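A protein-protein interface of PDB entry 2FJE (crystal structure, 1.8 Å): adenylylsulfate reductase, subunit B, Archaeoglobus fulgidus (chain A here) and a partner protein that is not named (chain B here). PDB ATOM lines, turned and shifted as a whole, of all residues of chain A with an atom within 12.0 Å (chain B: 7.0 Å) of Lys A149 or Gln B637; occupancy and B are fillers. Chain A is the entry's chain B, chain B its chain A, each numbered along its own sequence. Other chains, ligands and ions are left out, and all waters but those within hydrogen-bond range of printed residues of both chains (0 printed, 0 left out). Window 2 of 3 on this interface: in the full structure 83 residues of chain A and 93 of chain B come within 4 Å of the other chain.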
ATOM      1  N   GLN A 145      -8.234  -4.487  14.844  1.00  0.00           N
ATOM      2  CA  GLN A 145      -8.001  -3.060  15.035  1.00  0.00           C
ATOM      3  C   GLN A 145      -9.237  -2.300  14.566  1.00  0.00           C
ATOM      4  O   GLN A 145      -9.923  -2.730  13.639  1.00  0.00           O
ATOM      5  CB  GLN A 145      -6.785  -2.599  14.225  1.00  0.00           C
ATOM      6  CG  GLN A 145      -5.475  -3.246  14.640  1.00  0.00           C
ATOM      7  CD  GLN A 145      -5.083  -2.911  16.066  1.00  0.00           C
ATOM      8  OE1 GLN A 145      -4.859  -1.748  16.405  1.00  0.00           O
ATOM      9  NE2 GLN A 145      -5.000  -3.931  16.912  1.00  0.00           N
ATOM     10  N   VAL A 146      -9.525  -1.176  15.217  1.00  0.00           N
ATOM     11  CA  VAL A 146     -10.668  -0.350  14.843  1.00  0.00           C
ATOM     12  C   VAL A 146     -10.171   1.070  14.606  1.00  0.00           C
ATOM     13  O   VAL A 146      -9.429   1.615  15.418  1.00  0.00           O
ATOM     14  CB  VAL A 146     -11.733  -0.308  15.955  1.00  0.00           C
ATOM     15  CG1 VAL A 146     -13.037   0.250  15.402  1.00  0.00           C
ATOM     16  CG2 VAL A 146     -11.942  -1.694  16.534  1.00  0.00           C
ATOM     17  N   LYS A 147     -10.579   1.657  13.488  1.00  0.00           N
ATOM     18  CA  LYS A 147     -10.170   3.011  13.126  1.00  0.00           C
ATOM     19  C   LYS A 147     -10.803   4.063  14.064  1.00  0.00           C
ATOM     20  O   LYS A 147     -12.026   4.150  14.155  1.00  0.00           O
ATOM     21  CB  LYS A 147     -10.595   3.317  11.682  1.00  0.00           C
ATOM     22  CG  LYS A 147      -9.944   2.563  10.538  1.00  0.00           C
ATOM     23  CD  LYS A 147     -10.305   3.246   9.220  1.00  0.00           C
ATOM     24  CE  LYS A 147      -9.776   2.496   8.008  1.00  0.00           C
ATOM     25  NZ  LYS A 147     -10.491   1.205   7.794  1.00  0.00           N
ATOM     26  N   LYS A 148      -9.983   4.857  14.754  1.00  0.00           N
ATOM     27  CA  LYS A 148     -10.488   5.908  15.660  1.00  0.00           C
ATOM     28  C   LYS A 148     -10.862   7.162  14.855  1.00  0.00           C
ATOM     29  O   LYS A 148     -10.179   7.498  13.886  1.00  0.00           O
ATOM     30  CB  LYS A 148      -9.429   6.287  16.722  1.00  0.00           C
ATOM     31  CG  LYS A 148      -9.416   5.401  17.998  1.00  0.00           C
ATOM     32  CD  LYS A 148      -8.243   5.664  18.991  1.00  0.00           C
ATOM     33  CE  LYS A 148      -8.258   4.764  20.230  1.00  0.00           C
ATOM     34  NZ  LYS A 148      -7.196   5.140  21.229  1.00  0.00           N
ATOM     35  N   LYS A 149     -11.940   7.844  15.250  1.00  0.00           N
ATOM     36  CA  LYS A 149     -12.389   9.061  14.556  1.00  0.00           C
ATOM     37  C   LYS A 149     -11.264  10.089  14.528  1.00  0.00           C
ATOM     38  O   LYS A 149     -10.693  10.425  15.565  1.00  0.00           O
ATOM     39  CB  LYS A 149     -13.628   9.679  15.246  1.00  0.00           C
ATOM     40  CG  LYS A 149     -13.937  11.131  14.807  1.00  0.00           C
ATOM     41  CD  LYS A 149     -14.969  11.320  13.668  1.00  0.00           C
ATOM     42  CE  LYS A 149     -15.244  12.820  13.437  1.00  0.00           C
ATOM     43  NZ  LYS A 149     -16.473  13.153  12.658  1.00  0.00           N
ATOM     44  N   ALA A 150     -10.951  10.593  13.338  1.00  0.00           N
ATOM     45  CA  ALA A 150      -9.896  11.586  13.181  1.00  0.00           C
ATOM     46  C   ALA A 150     -10.373  12.959  13.647  1.00  0.00           C
ATOM     47  O   ALA A 150     -11.384  13.474  13.164  1.00  0.00           O
ATOM     48  CB  ALA A 150      -9.456  11.653  11.722  1.00  0.00           C
ATOM     49  N   VAL B  93     -20.085  -0.377  14.549  1.00  0.00           N
ATOM     50  CA  VAL B  93     -20.188   0.745  15.475  1.00  0.00           C
ATOM     51  C   VAL B  93     -21.163   1.775  14.908  1.00  0.00           C
ATOM     52  O   VAL B  93     -22.008   2.307  15.632  1.00  0.00           O
ATOM     53  CB  VAL B  93     -18.810   1.418  15.708  1.00  0.00           C
ATOM     54  CG1 VAL B  93     -18.973   2.663  16.577  1.00  0.00           C
ATOM     55  CG2 VAL B  93     -17.862   0.438  16.378  1.00  0.00           C
ATOM     56  N   THR B  97     -24.721   3.060  16.683  1.00  0.00           N
ATOM     57  CA  THR B  97     -24.922   4.465  17.014  1.00  0.00           C
ATOM     58  C   THR B  97     -26.160   4.992  16.298  1.00  0.00           C
ATOM     59  O   THR B  97     -26.979   5.689  16.893  1.00  0.00           O
ATOM     60  CB  THR B  97     -23.686   5.321  16.639  1.00  0.00           C
ATOM     61  OG1 THR B  97     -22.602   4.988  17.514  1.00  0.00           O
ATOM     62  CG2 THR B  97     -23.994   6.814  16.775  1.00  0.00           C
ATOM     63  N   ALA B 104     -24.619   6.523  21.552  1.00  0.00           N
ATOM     64  CA  ALA B 104     -24.047   5.260  22.005  1.00  0.00           C
ATOM     65  C   ALA B 104     -22.592   5.490  22.391  1.00  0.00           C
ATOM     66  O   ALA B 104     -21.905   6.297  21.766  1.00  0.00           O
ATOM     67  CB  ALA B 104     -24.136   4.215  20.901  1.00  0.00           C
ATOM     68  N   GLU B 106     -19.451   4.632  21.858  1.00  0.00           N
ATOM     69  CA  GLU B 106     -18.712   3.904  20.837  1.00  0.00           C
ATOM     70  C   GLU B 106     -17.458   3.203  21.338  1.00  0.00           C
ATOM     71  O   GLU B 106     -17.032   2.204  20.757  1.00  0.00           O
ATOM     72  CB  GLU B 106     -18.394   4.844  19.674  1.00  0.00           C
ATOM     73  CG  GLU B 106     -19.652   5.432  19.062  1.00  0.00           C
ATOM     74  CD  GLU B 106     -19.388   6.268  17.831  1.00  0.00           C
ATOM     75  OE1 GLU B 106     -18.228   6.686  17.631  1.00  0.00           O
ATOM     76  OE2 GLU B 106     -20.352   6.517  17.075  1.00  0.00           O
ATOM     77  N   PRO B 414     -12.387   7.992  25.242  1.00  0.00           N
ATOM     78  CA  PRO B 414     -11.904   9.372  25.146  1.00  0.00           C
ATOM     79  C   PRO B 414     -11.937  10.025  26.523  1.00  0.00           C
ATOM     80  O   PRO B 414     -12.676   9.587  27.406  1.00  0.00           O
ATOM     81  CB  PRO B 414     -12.908  10.035  24.200  1.00  0.00           C
ATOM     82  CG  PRO B 414     -13.562   8.887  23.483  1.00  0.00           C
ATOM     83  CD  PRO B 414     -13.679   7.849  24.554  1.00  0.00           C
ATOM     84  N   TYR B 417     -15.247  10.834  28.284  1.00  0.00           N
ATOM     85  CA  TYR B 417     -16.023   9.809  28.985  1.00  0.00           C
ATOM     86  C   TYR B 417     -15.396   9.255  30.265  1.00  0.00           C
ATOM     87  O   TYR B 417     -16.030   8.478  30.980  1.00  0.00           O
ATOM     88  CB  TYR B 417     -16.282   8.635  28.035  1.00  0.00           C
ATOM     89  CG  TYR B 417     -17.108   8.961  26.806  1.00  0.00           C
ATOM     90  CD1 TYR B 417     -17.121   8.095  25.710  1.00  0.00           C
ATOM     91  CD2 TYR B 417     -17.907  10.106  26.750  1.00  0.00           C
ATOM     92  CE1 TYR B 417     -17.910   8.355  24.593  1.00  0.00           C
ATOM     93  CE2 TYR B 417     -18.701  10.376  25.635  1.00  0.00           C
ATOM     94  CZ  TYR B 417     -18.697   9.494  24.561  1.00  0.00           C
ATOM     95  OH  TYR B 417     -19.482   9.740  23.459  1.00  0.00           O
ATOM     96  N   LYS B 614     -27.950  16.038  22.280  1.00  0.00           N
ATOM     97  CA  LYS B 614     -27.158  14.947  21.727  1.00  0.00           C
ATOM     98  C   LYS B 614     -26.128  14.638  22.803  1.00  0.00           C
ATOM     99  O   LYS B 614     -24.928  14.871  22.642  1.00  0.00           O
ATOM    100  CB  LYS B 614     -26.469  15.353  20.425  1.00  0.00           C
ATOM    101  CG  LYS B 614     -25.863  14.157  19.708  1.00  0.00           C
ATOM    102  CD  LYS B 614     -25.371  14.499  18.320  1.00  0.00           C
ATOM    103  CE  LYS B 614     -24.928  13.238  17.605  1.00  0.00           C
ATOM    104  NZ  LYS B 614     -24.428  13.513  16.225  1.00  0.00           N
ATOM    105  N   TYR B 635     -22.195  13.561  23.531  1.00  0.00           N
ATOM    106  CA  TYR B 635     -21.722  12.437  22.738  1.00  0.00           C
ATOM    107  C   TYR B 635     -20.586  12.924  21.856  1.00  0.00           C
ATOM    108  O   TYR B 635     -20.644  14.024  21.312  1.00  0.00           O
ATOM    109  CB  TYR B 635     -22.840  11.903  21.836  1.00  0.00           C
ATOM    110  CG  TYR B 635     -22.342  11.151  20.612  1.00  0.00           C
ATOM    111  CD1 TYR B 635     -22.203   9.761  20.620  1.00  0.00           C
ATOM    112  CD2 TYR B 635     -22.006  11.837  19.444  1.00  0.00           C
ATOM    113  CE1 TYR B 635     -21.745   9.073  19.486  1.00  0.00           C
ATOM    114  CE2 TYR B 635     -21.545  11.165  18.314  1.00  0.00           C
ATOM    115  CZ  TYR B 635     -21.418   9.788  18.339  1.00  0.00           C
ATOM    116  OH  TYR B 635     -20.975   9.139  17.206  1.00  0.00           O
ATOM    117  N   VAL B 636     -19.553  12.100  21.728  1.00  0.00           N
ATOM    118  CA  VAL B 636     -18.424  12.407  20.865  1.00  0.00           C
ATOM    119  C   VAL B 636     -18.235  11.166  20.000  1.00  0.00           C
ATOM    120  O   VAL B 636     -18.370  10.042  20.493  1.00  0.00           O
ATOM    121  CB  VAL B 636     -17.128  12.677  21.673  1.00  0.00           C
ATOM    122  CG1 VAL B 636     -17.283  13.945  22.497  1.00  0.00           C
ATOM    123  CG2 VAL B 636     -16.810  11.498  22.577  1.00  0.00           C
ATOM    124  N   GLN B 637     -17.964  11.354  18.714  1.00  0.00           N
ATOM    125  CA  GLN B 637     -17.763  10.207  17.840  1.00  0.00           C
ATOM    126  C   GLN B 637     -16.358   9.676  18.090  1.00  0.00           C
ATOM    127  O   GLN B 637     -15.373  10.376  17.850  1.00  0.00           O
ATOM    128  CB  GLN B 637     -17.911  10.604  16.372  1.00  0.00           C
ATOM    129  CG  GLN B 637     -18.024   9.399  15.442  1.00  0.00           C
ATOM    130  CD  GLN B 637     -18.187   9.785  13.987  1.00  0.00           C
ATOM    131  OE1 GLN B 637     -18.820  10.792  13.666  1.00  0.00           O
ATOM    132  NE2 GLN B 637     -17.637   8.970  13.094  1.00  0.00           N
ATOM    133  N   VAL B 638     -16.274   8.440  18.574  1.00  0.00           N
ATOM    134  CA  VAL B 638     -14.994   7.806  18.884  1.00  0.00           C
ATOM    135  C   VAL B 638     -14.406   7.029  17.709  1.00  0.00           C
ATOM    136  O   VAL B 638     -13.192   7.051  17.490  1.00  0.00           O
ATOM    137  CB  VAL B 638     -15.138   6.832  20.073  1.00  0.00           C
ATOM    138  CG1 VAL B 638     -13.788   6.226  20.421  1.00  0.00           C
ATOM    139  CG2 VAL B 638     -15.723   7.554  21.270  1.00  0.00           C
ATOM    140  N   ILE B 639     -15.268   6.343  16.965  1.00  0.00           N
ATOM    141  CA  ILE B 639     -14.838   5.539  15.825  1.00  0.00           C
ATOM    142  C   ILE B 639     -15.093   6.235  14.494  1.00  0.00           C
ATOM    143  O   ILE B 639     -16.066   6.970  14.333  1.00  0.00           O
ATOM    144  CB  ILE B 639     -15.555   4.161  15.803  1.00  0.00           C
ATOM    145  CG1 ILE B 639     -15.129   3.321  17.007  1.00  0.00           C
ATOM    146  CG2 ILE B 639     -15.210   3.405  14.523  1.00  0.00           C
ATOM    147  CD1 ILE B 639     -15.590   3.857  18.334  1.00  0.00           C
ATOM    148  N   GLU B 640     -14.208   5.986  13.537  1.00  0.00           N
ATOM    149  CA  GLU B 640     -14.318   6.583  12.215  1.00  0.00           C
ATOM    150  C   GLU B 640     -15.412   5.929  11.368  1.00  0.00           C
ATOM    151  O   GLU B 640     -15.392   4.720  11.137  1.00  0.00           O
ATOM    152  CB  GLU B 640     -12.971   6.474  11.495  1.00  0.00           C
ATOM    153  CG  GLU B 640     -12.948   7.064  10.100  1.00  0.00           C
ATOM    154  CD  GLU B 640     -11.631   6.811   9.393  1.00  0.00           C
ATOM    155  OE1 GLU B 640     -10.586   7.269   9.904  1.00  0.00           O
ATOM    156  OE2 GLU B 640     -11.639   6.150   8.332  1.00  0.00           O
ATOM    157  N   TRP B 641     -16.368   6.738  10.925  1.00  0.00           N
ATOM    158  CA  TRP B 641     -17.464   6.286  10.074  1.00  0.00           C
ATOM    159  C   TRP B 641     -18.252   7.485   9.566  1.00  0.00           C
ATOM    160  O   TRP B 641     -18.181   8.571  10.142  1.00  0.00           O
ATOM    161  CB  TRP B 641     -18.408   5.321  10.816  1.00  0.00           C
ATOM    162  CG  TRP B 641     -19.107   5.887  12.030  1.00  0.00           C
ATOM    163  CD1 TRP B 641     -18.743   5.721  13.339  1.00  0.00           C
ATOM    164  CD2 TRP B 641     -20.298   6.681  12.046  1.00  0.00           C
ATOM    165  NE1 TRP B 641     -19.636   6.358  14.167  1.00  0.00           N
ATOM    166  CE2 TRP B 641     -20.601   6.956  13.399  1.00  0.00           C
ATOM    167  CE3 TRP B 641     -21.143   7.187  11.047  1.00  0.00           C
ATOM    168  CZ2 TRP B 641     -21.711   7.717  13.779  1.00  0.00           C
ATOM    169  CZ3 TRP B 641     -22.248   7.943  11.426  1.00  0.00           C
ATOM    170  CH2 TRP B 641     -22.521   8.201  12.781  1.00  0.00           C
ATOM    171  N   SER B 642     -18.995   7.288   8.481  1.00  0.00           N
ATOM    172  CA  SER B 642     -19.804   8.352   7.893  1.00  0.00           C
ATOM    173  C   SER B 642     -21.187   7.814   7.548  1.00  0.00           C
ATOM    174  O   SER B 642     -21.357   6.612   7.356  1.00  0.00           O
ATOM    175  CB  SER B 642     -19.136   8.888   6.623  1.00  0.00           C
ATOM    176  OG  SER B 642     -17.853   9.422   6.902  1.00  0.00           O
ATOM    177  N   PHE B 643     -22.174   8.702   7.466  1.00  0.00           N
ATOM    178  CA  PHE B 643     -23.532   8.286   7.133  1.00  0.00           C
ATOM    179  C   PHE B 643     -23.591   7.776   5.697  1.00  0.00           C
ATOM    180  O   PHE B 643     -23.697   6.573   5.458  1.00  0.00           O
ATOM    181  CB  PHE B 643     -24.515   9.448   7.294  1.00  0.00           C
ATOM    182  CG  PHE B 643     -24.545  10.037   8.678  1.00  0.00           C
ATOM    183  CD1 PHE B 643     -23.699  11.087   9.021  1.00  0.00           C
ATOM    184  CD2 PHE B 643     -25.420   9.541   9.639  1.00  0.00           C
ATOM    185  CE1 PHE B 643     -23.724  11.636  10.304  1.00  0.00           C
ATOM    186  CE2 PHE B 643     -25.452  10.082  10.926  1.00  0.00           C
ATOM    187  CZ  PHE B 643     -24.603  11.132  11.257  1.00  0.00           C
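Of the 6 printed residues of chain A, 4 touch a printed residue of chain B. Hydrophobic or aromatic side chains of chain A within 4 Å of the printed part of chain B: Val A146. Hydrophobic or aromatic side chains of chain B within 4 Å of the printed part of chain A: Ile B639. Among the printed residues, 9 pairs touch across the chains. Among the printed residues, no Asp or Glu carboxylate lies within 4 Å of a Lys or Arg side-chain nitrogen of the other chain.
The side-chain amide oxygen (OE1) of Gln B637 sits at hydrogen-bond distance from the side-chain amino group (NZ) of Lys A149 (3.5 Å). The backbone carbonyl oxygen (O) of Val B638 is in hydrogen-bond range of the backbone NH (N) of Lys A149 (2.7 Å). The backbone NH (N) of Glu B640 is in hydrogen-bond range of the backbone carbonyl oxygen (O) of Lys A147. The backbone NH (N) of Lys A149 lies close to the backbone NH (N) of Glu B640 (3.4 Å).
Of the printed residues of chain B, Val A146 touches Ile B639 (3.9 Å). Printed residues of chain B within 4 Å of Lys A147: Ile B639 and Glu B640. Printed residues of chain B within 4 Å of Lys A148: Val B638 and Glu B640. No residue of chain A comes within 4 Å of Tyr B635. Printed residues of chain A within 4 Å of Gln B637: Lys A149 (3.2 Å). Val B638 touches two residues of chain A. Of chain A, only Val A146 (3.9 Å), Lys A147 (3.3 Å) and Lys A149 (3.6 Å) come within 4 Å of Ile B639. Of chain A, only Lys A147, Lys A148 and Lys A149 come within 4 Å of Glu B640. No residue of chain A comes within 4 Å of Trp B641. No residue of chain A comes within 4 Å of Ser B642. The nearest printed residue of chain A that does not touch Gln B637 is Lys A148 (6.3 Å). The nearest printed residue of chain B that does not touch Lys A147 is Val B638 (4.6 Å).
The side-chain carboxylate (OE1) of Glu B106 is in hydrogen-bond range of the backbone NH (N) of Val B638 (2.8 Å). OE1 of Glu B106 lies within hydrogen-bond range of N of Ile B639 (3.1 Å). O of Ile B639 sits at hydrogen-bond distance from NE2 of Gln B637, 2.8 Å away. The side-chain amide nitrogen (NE2) of Gln B637 sits at hydrogen-bond distance from the backbone carbonyl oxygen (O) of Trp B641 (3.0 Å).
CG1 of Val A146 touches CG2 of Ile B639, at 3.9 Å. Lys A147 touches Ile B639 (O to CG2, 3.3 Å). O of Val B638 touches CA of Lys A148, 3.5 Å away. C of Lys A148 touches N of Glu B640 (3.8 Å). Lys A149 touches Ile B639.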
